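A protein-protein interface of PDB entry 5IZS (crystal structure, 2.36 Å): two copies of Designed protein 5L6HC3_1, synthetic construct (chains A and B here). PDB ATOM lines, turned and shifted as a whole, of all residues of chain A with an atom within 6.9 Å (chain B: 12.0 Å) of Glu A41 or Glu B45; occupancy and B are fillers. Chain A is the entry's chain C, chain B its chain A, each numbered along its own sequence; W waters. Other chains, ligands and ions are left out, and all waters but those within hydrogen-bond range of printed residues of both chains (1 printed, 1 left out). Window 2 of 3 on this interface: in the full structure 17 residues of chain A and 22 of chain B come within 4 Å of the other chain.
The guanidinium group (NH1) of Arg B49 is in salt-bridge range of the side-chain carboxylate (OE2) of Glu A41 (3.1 Å). The side-chain carboxylate (OE2) of Glu B45 sits at hydrogen-bond distance from the side-chain hydroxyl (OG) of Ser A40 (2.8 Å).
Water W1 bridges OE1 of Glu B45 (2.4 Å) and O of Ser A40 (2.8 Å).
The side-chain carboxylate (OE2) of Glu B45 lies within salt-bridge range of the guanidinium group (NH2) of Arg B49, at 3.9 Å. OD1 of Asp A34 lies within salt-bridge range of NH1 of Arg A37, at 2.8 Å. O of Arg A37 lies within hydrogen-bond range of OG of Ser A40, 2.8 Å away. The backbone carbonyl oxygen (O) of Leu B35 is in hydrogen-bond range of the side-chain hydroxyl (OG1) of Thr B39 (2.7 Å).
Along chain B the printed residues that touch a printed residue of chain A span positions 39 to 52. Printed residues of chain A that touch a printed residue of chain B: Val A36, Arg A37, Ser A40 and Glu A41. Among the printed residues, 6 pairs touch across the chains. Among the printed residues, Asp or Glu carboxylates within 4 Å of a Lys or Arg side-chain nitrogen of the other chain: Glu A41 with Arg B49.
Arg A37 touches just one residue of chain B: Ile B52 (3.6 Å). No residue of chain B comes within 4 Å of Lys A38. No residue of chain B comes within 4 Å of Thr A39. Glu A41 touches just these residues of chain B: Glu B45 and Arg B49. No residue of chain B comes within 4 Å of Leu A42. No residue of chain B comes within 4 Å of Thr A43. Of the printed residues of chain A, Thr B39 touches Val A36 (3.99 Å). Glu B45 touches two residues of chain A. Of the printed residues of chain A, Ile B52 touches Arg A37 (3.6 Å). The nearest residue of chain B that does not touch Glu A41 is Ile B48 (6.9 Å).
Val A36 touches Thr B39, but with the chains exchanged Thr A39 does not touch Val B36 (8.2 Å). Ser A40 touches Ile B48, but with the chains exchanged Ile A48 does not touch Ser B40 (12.3 Å). Of the 6 pairs that touch across the chains among the printed residues, none has its exchanged pair printed and touching as well.
Val A36 touches Thr B39. NH2 of Arg A37 touches CG2 of Ile B52, 3.6 Å away. Ile B48 touches Ser A40. Glu A41 touches Glu B45.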
ATOM      1  N   ASP A  34     -18.410   2.565 -31.954  1.00  0.00           N
ATOM      2  CA  ASP A  34     -17.341   1.646 -31.566  1.00  0.00           C
ATOM      3  C   ASP A  34     -16.361   2.310 -30.598  1.00  0.00           C
ATOM      4  O   ASP A  34     -15.908   1.687 -29.637  1.00  0.00           O
ATOM      5  CB  ASP A  34     -16.586   1.138 -32.798  1.00  0.00           C
ATOM      6  CG  ASP A  34     -17.442   0.251 -33.690  1.00  0.00           C
ATOM      7  OD1 ASP A  34     -18.403  -0.368 -33.183  1.00  0.00           O
ATOM      8  OD2 ASP A  34     -17.155   0.175 -34.905  1.00  0.00           O
ATOM      9  N   VAL A  36     -17.001   4.786 -28.543  1.00  0.00           N
ATOM     10  CA  VAL A  36     -17.689   4.944 -27.266  1.00  0.00           C
ATOM     11  C   VAL A  36     -17.798   3.604 -26.540  1.00  0.00           C
ATOM     12  O   VAL A  36     -17.671   3.543 -25.316  1.00  0.00           O
ATOM     13  CB  VAL A  36     -19.093   5.553 -27.454  1.00  0.00           C
ATOM     14  CG1 VAL A  36     -19.835   5.620 -26.129  1.00  0.00           C
ATOM     15  CG2 VAL A  36     -18.985   6.936 -28.072  1.00  0.00           C
ATOM     16  N   ARG A  37     -18.029   2.532 -27.296  1.00  0.00           N
ATOM     17  CA  ARG A  37     -18.101   1.198 -26.709  1.00  0.00           C
ATOM     18  C   ARG A  37     -16.779   0.821 -26.051  1.00  0.00           C
ATOM     19  O   ARG A  37     -16.749   0.410 -24.893  1.00  0.00           O
ATOM     20  CB  ARG A  37     -18.465   0.148 -27.757  1.00  0.00           C
ATOM     21  CG  ARG A  37     -18.444  -1.271 -27.194  1.00  0.00           C
ATOM     22  CD  ARG A  37     -18.751  -2.326 -28.246  1.00  0.00           C
ATOM     23  NE  ARG A  37     -20.077  -2.164 -28.834  1.00  0.00           N
ATOM     24  CZ  ARG A  37     -20.290  -1.877 -30.113  1.00  0.00           C
ATOM     25  NH1 ARG A  37     -19.261  -1.728 -30.937  1.00  0.00           N
ATOM     26  NH2 ARG A  37     -21.529  -1.747 -30.572  1.00  0.00           N
ATOM     27  N   LYS A  38     -15.689   0.965 -26.796  1.00  0.00           N
ATOM     28  CA  LYS A  38     -14.364   0.626 -26.293  1.00  0.00           C
ATOM     29  C   LYS A  38     -13.945   1.554 -25.154  1.00  0.00           C
ATOM     30  O   LYS A  38     -13.208   1.155 -24.256  1.00  0.00           O
ATOM     31  CB  LYS A  38     -13.333   0.675 -27.423  1.00  0.00           C
ATOM     32  CG  LYS A  38     -13.464  -0.461 -28.433  1.00  0.00           C
ATOM     33  CD  LYS A  38     -12.509  -0.294 -29.610  1.00  0.00           C
ATOM     34  CE  LYS A  38     -12.637  -1.449 -30.597  1.00  0.00           C
ATOM     35  NZ  LYS A  38     -11.751  -1.294 -31.786  1.00  0.00           N
ATOM     36  N   THR A  39     -14.427   2.792 -25.185  1.00  0.00           N
ATOM     37  CA  THR A  39     -14.079   3.763 -24.152  1.00  0.00           C
ATOM     38  C   THR A  39     -14.654   3.376 -22.790  1.00  0.00           C
ATOM     39  O   THR A  39     -14.002   3.565 -21.759  1.00  0.00           O
ATOM     40  CB  THR A  39     -14.563   5.174 -24.516  1.00  0.00           C
ATOM     41  OG1 THR A  39     -13.626   5.781 -25.414  1.00  0.00           O
ATOM     42  N   SER A  40     -15.871   2.840 -22.790  1.00  0.00           N
ATOM     43  CA  SER A  40     -16.509   2.390 -21.559  1.00  0.00           C
ATOM     44  C   SER A  40     -15.849   1.112 -21.043  1.00  0.00           C
ATOM     45  O   SER A  40     -15.845   0.843 -19.842  1.00  0.00           O
ATOM     46  CB  SER A  40     -18.003   2.151 -21.782  1.00  0.00           C
ATOM     47  OG  SER A  40     -18.217   1.037 -22.637  1.00  0.00           O
ATOM     48  N   GLU A  41     -15.279   0.339 -21.963  1.00  0.00           N
ATOM     49  CA  GLU A  41     -14.689  -0.960 -21.642  1.00  0.00           C
ATOM     50  C   GLU A  41     -13.280  -0.844 -21.057  1.00  0.00           C
ATOM     51  O   GLU A  41     -12.862  -1.681 -20.258  1.00  0.00           O
ATOM     52  CB  GLU A  41     -14.651  -1.844 -22.894  1.00  0.00           C
ATOM     53  CG  GLU A  41     -16.012  -2.306 -23.406  1.00  0.00           C
ATOM     54  CD  GLU A  41     -15.942  -2.880 -24.816  1.00  0.00           C
ATOM     55  OE1 GLU A  41     -14.947  -2.608 -25.519  1.00  0.00           O
ATOM     56  OE2 GLU A  41     -16.876  -3.604 -25.223  1.00  0.00           O
ATOM     57  N   LEU A  42     -12.553   0.196 -21.455  1.00  0.00           N
ATOM     58  CA  LEU A  42     -11.148   0.337 -21.083  1.00  0.00           C
ATOM     59  C   LEU A  42     -10.924   1.364 -19.974  1.00  0.00           C
ATOM     60  O   LEU A  42     -11.662   2.341 -19.862  1.00  0.00           O
ATOM     61  CB  LEU A  42     -10.323   0.723 -22.312  1.00  0.00           C
ATOM     62  CG  LEU A  42     -10.493  -0.173 -23.541  1.00  0.00           C
ATOM     63  CD1 LEU A  42     -10.084   0.557 -24.815  1.00  0.00           C
ATOM     64  CD2 LEU A  42      -9.712  -1.469 -23.377  1.00  0.00           C
ATOM     65  N   THR A  43      -9.893   1.139 -19.166  1.00  0.00           N
ATOM     66  CA  THR A  43      -9.499   2.087 -18.126  1.00  0.00           C
ATOM     67  C   THR A  43      -8.072   2.602 -18.326  1.00  0.00           C
ATOM     68  O   THR A  43      -7.714   3.657 -17.804  1.00  0.00           O
ATOM     69  CB  THR A  43      -9.615   1.467 -16.722  1.00  0.00           C
ATOM     70  OG1 THR A  43      -9.042   0.151 -16.731  1.00  0.00           O
ATOM     71  CG2 THR A  43     -11.076   1.377 -16.295  1.00  0.00           C
ATOM     72  N   ASP A  44      -7.260   1.864 -19.080  1.00  0.00           N
ATOM     73  CA  ASP A  44      -5.918   2.333 -19.415  1.00  0.00           C
ATOM     74  C   ASP A  44      -6.012   3.464 -20.433  1.00  0.00           C
ATOM     75  O   ASP A  44      -6.452   3.263 -21.561  1.00  0.00           O
ATOM     76  CB  ASP A  44      -5.050   1.193 -19.961  1.00  0.00           C
ATOM     77  CG  ASP A  44      -3.571   1.565 -20.046  1.00  0.00           C
ATOM     78  OD1 ASP A  44      -3.248   2.764 -20.189  1.00  0.00           O
ATOM     79  OD2 ASP A  44      -2.722   0.650 -19.971  1.00  0.00           O
ATOM     80  N   ILE A  48      -6.882   3.845 -24.491  1.00  0.00           N
ATOM     81  CA  ILE A  48      -7.989   4.690 -24.927  1.00  0.00           C
ATOM     82  C   ILE A  48      -7.536   5.754 -25.930  1.00  0.00           C
ATOM     83  O   ILE A  48      -8.207   5.996 -26.935  1.00  0.00           O
ATOM     84  CB  ILE A  48      -8.664   5.365 -23.714  1.00  0.00           C
ATOM     85  CG1 ILE A  48      -9.392   4.320 -22.869  1.00  0.00           C
ATOM     86  CG2 ILE A  48      -9.640   6.442 -24.157  1.00  0.00           C
ATOM     87  CD1 ILE A  48      -9.878   4.846 -21.543  1.00  0.00           C
ATOM     88  N   LEU B  35     -25.604   9.573 -26.632  1.00  0.00           N
ATOM     89  CA  LEU B  35     -24.936   8.339 -26.225  1.00  0.00           C
ATOM     90  C   LEU B  35     -23.761   8.644 -25.300  1.00  0.00           C
ATOM     91  O   LEU B  35     -23.538   7.948 -24.312  1.00  0.00           O
ATOM     92  CB  LEU B  35     -24.457   7.548 -27.443  1.00  0.00           C
ATOM     93  CG  LEU B  35     -23.774   6.217 -27.117  1.00  0.00           C
ATOM     94  CD1 LEU B  35     -24.735   5.302 -26.374  1.00  0.00           C
ATOM     95  CD2 LEU B  35     -23.238   5.539 -28.374  1.00  0.00           C
ATOM     96  N   VAL B  36     -23.019   9.697 -25.625  1.00  0.00           N
ATOM     97  CA  VAL B  36     -21.906  10.140 -24.796  1.00  0.00           C
ATOM     98  C   VAL B  36     -22.387  10.680 -23.449  1.00  0.00           C
ATOM     99  O   VAL B  36     -21.765  10.423 -22.416  1.00  0.00           O
ATOM    100  CB  VAL B  36     -21.072  11.216 -25.514  1.00  0.00           C
ATOM    101  CG1 VAL B  36     -20.102  11.888 -24.553  1.00  0.00           C
ATOM    102  CG2 VAL B  36     -20.330  10.600 -26.689  1.00  0.00           C
ATOM    103  N   LYS B  38     -25.294   9.941 -21.805  1.00  0.00           N
ATOM    104  CA  LYS B  38     -25.842   8.872 -20.984  1.00  0.00           C
ATOM    105  C   LYS B  38     -24.730   7.964 -20.462  1.00  0.00           C
ATOM    106  O   LYS B  38     -24.748   7.564 -19.303  1.00  0.00           O
ATOM    107  CB  LYS B  38     -26.874   8.056 -21.767  1.00  0.00           C
ATOM    108  CG  LYS B  38     -28.071   8.861 -22.265  1.00  0.00           C
ATOM    109  CD  LYS B  38     -29.307   7.985 -22.420  1.00  0.00           C
ATOM    110  CE  LYS B  38     -30.281   8.530 -23.456  1.00  0.00           C
ATOM    111  NZ  LYS B  38     -29.848   8.251 -24.858  1.00  0.00           N
ATOM    112  N   THR B  39     -23.748   7.661 -21.307  1.00  0.00           N
ATOM    113  CA  THR B  39     -22.636   6.802 -20.904  1.00  0.00           C
ATOM    114  C   THR B  39     -21.821   7.432 -19.770  1.00  0.00           C
ATOM    115  O   THR B  39     -21.378   6.736 -18.852  1.00  0.00           O
ATOM    116  CB  THR B  39     -21.703   6.493 -22.092  1.00  0.00           C
ATOM    117  OG1 THR B  39     -22.424   5.763 -23.094  1.00  0.00           O
ATOM    118  CG2 THR B  39     -20.500   5.670 -21.633  1.00  0.00           C
ATOM    119  N   SER B  40     -21.629   8.747 -19.833  1.00  0.00           N
ATOM    120  CA  SER B  40     -20.926   9.468 -18.775  1.00  0.00           C
ATOM    121  C   SER B  40     -21.716   9.414 -17.469  1.00  0.00           C
ATOM    122  O   SER B  40     -21.143   9.461 -16.380  1.00  0.00           O
ATOM    123  CB  SER B  40     -20.690  10.925 -19.174  1.00  0.00           C
ATOM    124  OG  SER B  40     -21.829  11.721 -18.879  1.00  0.00           O
ATOM    125  N   GLU B  41     -23.036   9.311 -17.592  1.00  0.00           N
ATOM    126  CA  GLU B  41     -23.933   9.299 -16.440  1.00  0.00           C
ATOM    127  C   GLU B  41     -24.007   7.920 -15.781  1.00  0.00           C
ATOM    128  O   GLU B  41     -24.212   7.817 -14.571  1.00  0.00           O
ATOM    129  CB  GLU B  41     -25.334   9.765 -16.856  1.00  0.00           C
ATOM    130  CG  GLU B  41     -25.476  11.281 -16.990  1.00  0.00           C
ATOM    131  CD  GLU B  41     -26.614  11.703 -17.912  1.00  0.00           C
ATOM    132  OE1 GLU B  41     -27.343  10.823 -18.413  1.00  0.00           O
ATOM    133  OE2 GLU B  41     -26.776  12.920 -18.145  1.00  0.00           O
ATOM    134  N   LEU B  42     -23.821   6.865 -16.570  1.00  0.00           N
ATOM    135  CA  LEU B  42     -23.945   5.499 -16.066  1.00  0.00           C
ATOM    136  C   LEU B  42     -22.590   4.870 -15.737  1.00  0.00           C
ATOM    137  O   LEU B  42     -21.584   5.167 -16.384  1.00  0.00           O
ATOM    138  CB  LEU B  42     -24.683   4.629 -17.085  1.00  0.00           C
ATOM    139  CG  LEU B  42     -25.946   5.224 -17.719  1.00  0.00           C
ATOM    140  CD1 LEU B  42     -26.361   4.446 -18.965  1.00  0.00           C
ATOM    141  CD2 LEU B  42     -27.088   5.297 -16.713  1.00  0.00           C
ATOM    142  N   THR B  43     -22.578   3.990 -14.738  1.00  0.00           N
ATOM    143  CA  THR B  43     -21.379   3.244 -14.354  1.00  0.00           C
ATOM    144  C   THR B  43     -21.518   1.759 -14.697  1.00  0.00           C
ATOM    145  O   THR B  43     -20.538   1.092 -15.027  1.00  0.00           O
ATOM    146  CB  THR B  43     -21.070   3.388 -12.842  1.00  0.00           C
ATOM    147  OG1 THR B  43     -22.221   3.010 -12.074  1.00  0.00           O
ATOM    148  CG2 THR B  43     -20.689   4.825 -12.501  1.00  0.00           C
ATOM    149  N   ASP B  44     -22.746   1.250 -14.623  1.00  0.00           N
ATOM    150  CA  ASP B  44     -23.040  -0.143 -14.951  1.00  0.00           C
ATOM    151  C   ASP B  44     -22.859  -0.429 -16.442  1.00  0.00           C
ATOM    152  O   ASP B  44     -23.556   0.133 -17.282  1.00  0.00           O
ATOM    153  CB  ASP B  44     -24.469  -0.491 -14.523  1.00  0.00           C
ATOM    154  CG  ASP B  44     -24.754  -1.985 -14.567  1.00  0.00           C
ATOM    155  OD1 ASP B  44     -23.952  -2.747 -15.149  1.00  0.00           O
ATOM    156  OD2 ASP B  44     -25.796  -2.401 -14.020  1.00  0.00           O
ATOM    157  N   GLU B  45     -21.943  -1.340 -16.753  1.00  0.00           N
ATOM    158  CA  GLU B  45     -21.559  -1.626 -18.131  1.00  0.00           C
ATOM    159  C   GLU B  45     -22.639  -2.376 -18.912  1.00  0.00           C
ATOM    160  O   GLU B  45     -22.822  -2.140 -20.107  1.00  0.00           O
ATOM    161  CB  GLU B  45     -20.254  -2.420 -18.154  1.00  0.00           C
ATOM    162  CG  GLU B  45     -19.668  -2.610 -19.539  1.00  0.00           C
ATOM    163  CD  GLU B  45     -19.305  -1.298 -20.210  1.00  0.00           C
ATOM    164  OE1 GLU B  45     -19.153  -0.277 -19.504  1.00  0.00           O
ATOM    165  OE2 GLU B  45     -19.172  -1.291 -21.450  1.00  0.00           O
ATOM    166  N   LYS B  46     -23.340  -3.288 -18.238  1.00  0.00           N
ATOM    167  CA  LYS B  46     -24.487  -3.966 -18.829  1.00  0.00           C
ATOM    168  C   LYS B  46     -25.501  -2.928 -19.289  1.00  0.00           C
ATOM    169  O   LYS B  46     -26.024  -3.001 -20.397  1.00  0.00           O
ATOM    170  CB  LYS B  46     -25.125  -4.932 -17.828  1.00  0.00           C
ATOM    171  CG  LYS B  46     -26.522  -5.407 -18.212  1.00  0.00           C
ATOM    172  CD  LYS B  46     -27.165  -6.208 -17.085  1.00  0.00           C
ATOM    173  CE  LYS B  46     -28.625  -6.540 -17.388  1.00  0.00           C
ATOM    174  NZ  LYS B  46     -28.783  -7.607 -18.417  1.00  0.00           N
ATOM    175  N   THR B  47     -25.743  -1.944 -18.432  1.00  0.00           N
ATOM    176  CA  THR B  47     -26.675  -0.861 -18.713  1.00  0.00           C
ATOM    177  C   THR B  47     -26.178   0.051 -19.838  1.00  0.00           C
ATOM    178  O   THR B  47     -26.952   0.500 -20.684  1.00  0.00           O
ATOM    179  CB  THR B  47     -26.918  -0.024 -17.448  1.00  0.00           C
ATOM    180  OG1 THR B  47     -27.412  -0.872 -16.403  1.00  0.00           O
ATOM    181  CG2 THR B  47     -27.909   1.093 -17.718  1.00  0.00           C
ATOM    182  N   ILE B  48     -24.878   0.325 -19.826  1.00  0.00           N
ATOM    183  CA  ILE B  48     -24.238   1.135 -20.856  1.00  0.00           C
ATOM    184  C   ILE B  48     -24.333   0.449 -22.222  1.00  0.00           C
ATOM    185  O   ILE B  48     -24.476   1.110 -23.254  1.00  0.00           O
ATOM    186  CB  ILE B  48     -22.759   1.414 -20.488  1.00  0.00           C
ATOM    187  CG1 ILE B  48     -22.684   2.448 -19.364  1.00  0.00           C
ATOM    188  CG2 ILE B  48     -21.965   1.914 -21.689  1.00  0.00           C
ATOM    189  CD1 ILE B  48     -21.455   2.310 -18.497  1.00  0.00           C
ATOM    190  N   ARG B  49     -24.287  -0.880 -22.218  1.00  0.00           N
ATOM    191  CA  ARG B  49     -24.340  -1.655 -23.457  1.00  0.00           C
ATOM    192  C   ARG B  49     -25.703  -1.579 -24.144  1.00  0.00           C
ATOM    193  O   ARG B  49     -25.792  -1.681 -25.368  1.00  0.00           O
ATOM    194  CB  ARG B  49     -23.985  -3.121 -23.195  1.00  0.00           C
ATOM    195  CG  ARG B  49     -22.502  -3.372 -22.980  1.00  0.00           C
ATOM    196  CD  ARG B  49     -22.159  -4.852 -23.059  1.00  0.00           C
ATOM    197  NE  ARG B  49     -20.820  -5.110 -22.538  1.00  0.00           N
ATOM    198  CZ  ARG B  49     -19.698  -4.726 -23.137  1.00  0.00           C
ATOM    199  NH1 ARG B  49     -19.751  -4.065 -24.286  1.00  0.00           N
ATOM    200  NH2 ARG B  49     -18.522  -5.001 -22.587  1.00  0.00           N
ATOM    201  N   GLU B  50     -26.761  -1.402 -23.357  1.00  0.00           N
ATOM    202  CA  GLU B  50     -28.111  -1.322 -23.905  1.00  0.00           C
ATOM    203  C   GLU B  50     -28.314   0.022 -24.587  1.00  0.00           C
ATOM    204  O   GLU B  50     -28.948   0.104 -25.636  1.00  0.00           O
ATOM    205  CB  GLU B  50     -29.157  -1.524 -22.812  1.00  0.00           C
ATOM    206  CG  GLU B  50     -28.719  -2.502 -21.740  1.00  0.00           C
ATOM    207  CD  GLU B  50     -29.867  -3.024 -20.901  1.00  0.00           C
ATOM    208  OE1 GLU B  50     -30.863  -2.291 -20.722  1.00  0.00           O
ATOM    209  OE2 GLU B  50     -29.776  -4.177 -20.428  1.00  0.00           O
ATOM    210  N   GLU B  51     -27.764   1.071 -23.982  1.00  0.00           N
ATOM    211  CA  GLU B  51     -27.782   2.406 -24.570  1.00  0.00           C
ATOM    212  C   GLU B  51     -27.079   2.405 -25.926  1.00  0.00           C
ATOM    213  O   GLU B  51     -27.584   2.954 -26.905  1.00  0.00           O
ATOM    214  CB  GLU B  51     -27.115   3.415 -23.634  1.00  0.00           C
ATOM    215  CG  GLU B  51     -27.832   3.609 -22.309  1.00  0.00           C
ATOM    216  CD  GLU B  51     -29.190   4.264 -22.467  1.00  0.00           C
ATOM    217  OE1 GLU B  51     -29.417   4.937 -23.496  1.00  0.00           O
ATOM    218  OE2 GLU B  51     -30.035   4.098 -21.563  1.00  0.00           O
ATOM    219  N   ILE B  52     -25.904   1.787 -25.963  1.00  0.00           N
ATOM    220  CA  ILE B  52     -25.128   1.642 -27.191  1.00  0.00           C
ATOM    221  C   ILE B  52     -25.871   0.814 -28.237  1.00  0.00           C
ATOM    222  O   ILE B  52     -25.957   1.206 -29.399  1.00  0.00           O
ATOM    223  CB  ILE B  52     -23.760   1.003 -26.900  1.00  0.00           C
ATOM    224  CG1 ILE B  52     -22.821   2.035 -26.275  1.00  0.00           C
ATOM    225  CG2 ILE B  52     -23.148   0.427 -28.171  1.00  0.00           C
ATOM    226  CD1 ILE B  52     -21.700   1.420 -25.476  1.00  0.00           C
ATOM    227  N   ARG B  53     -26.414  -0.327 -27.815  1.00  0.00           N
ATOM    228  CA  ARG B  53     -27.180  -1.191 -28.708  1.00  0.00           C
ATOM    229  C   ARG B  53     -28.414  -0.471 -29.256  1.00  0.00           C
ATOM    230  O   ARG B  53     -28.806  -0.680 -30.404  1.00  0.00           O
ATOM    231  CB  ARG B  53     -27.595  -2.471 -27.982  1.00  0.00           C
ATOM    232  CG  ARG B  53     -28.046  -3.596 -28.899  1.00  0.00           C
ATOM    233  CD  ARG B  53     -26.972  -3.919 -29.923  1.00  0.00           C
ATOM    234  NE  ARG B  53     -27.259  -5.143 -30.665  1.00  0.00           N
ATOM    235  CZ  ARG B  53     -28.245  -5.267 -31.546  1.00  0.00           C
ATOM    236  NH1 ARG B  53     -29.049  -4.242 -31.784  1.00  0.00           N
ATOM    237  NH2 ARG B  53     -28.436  -6.416 -32.178  1.00  0.00           N
ATOM    238  N   LYS B  54     -29.009   0.389 -28.434  1.00  0.00           N
ATOM    239  CA  LYS B  54     -30.206   1.133 -28.818  1.00  0.00           C
ATOM    240  C   LYS B  54     -29.883   2.252 -29.807  1.00  0.00           C
ATOM    241  O   LYS B  54     -30.592   2.442 -30.790  1.00  0.00           O
ATOM    242  CB  LYS B  54     -30.890   1.714 -27.580  1.00  0.00           C
ATOM    243  CG  LYS B  54     -32.272   2.292 -27.836  1.00  0.00           C
ATOM    244  CD  LYS B  54     -32.672   3.225 -26.706  1.00  0.00           C
ATOM    245  CE  LYS B  54     -31.666   4.363 -26.568  1.00  0.00           C
ATOM    246  NZ  LYS B  54     -31.953   5.261 -25.416  1.00  0.00           N
ATOM    247  N   LYS B  56     -27.285   2.288 -31.770  1.00  0.00           N
ATOM    248  CA  LYS B  56     -26.819   1.623 -32.982  1.00  0.00           C
ATOM    249  C   LYS B  56     -27.962   1.273 -33.937  1.00  0.00           C
ATOM    250  O   LYS B  56     -27.902   1.595 -35.125  1.00  0.00           O
ATOM    251  CB  LYS B  56     -26.037   0.359 -32.621  1.00  0.00           C
ATOM    252  CG  LYS B  56     -25.615  -0.479 -33.818  1.00  0.00           C
ATOM    253  CD  LYS B  56     -24.424  -1.369 -33.483  1.00  0.00           C
ATOM    254  CE  LYS B  56     -24.172  -2.398 -34.583  1.00  0.00           C
ATOM    255  NZ  LYS B  56     -23.135  -3.401 -34.200  1.00  0.00           N
HETATM  256  O   HOH W   1     -17.784   0.748 -17.761  1.00  0.00           O
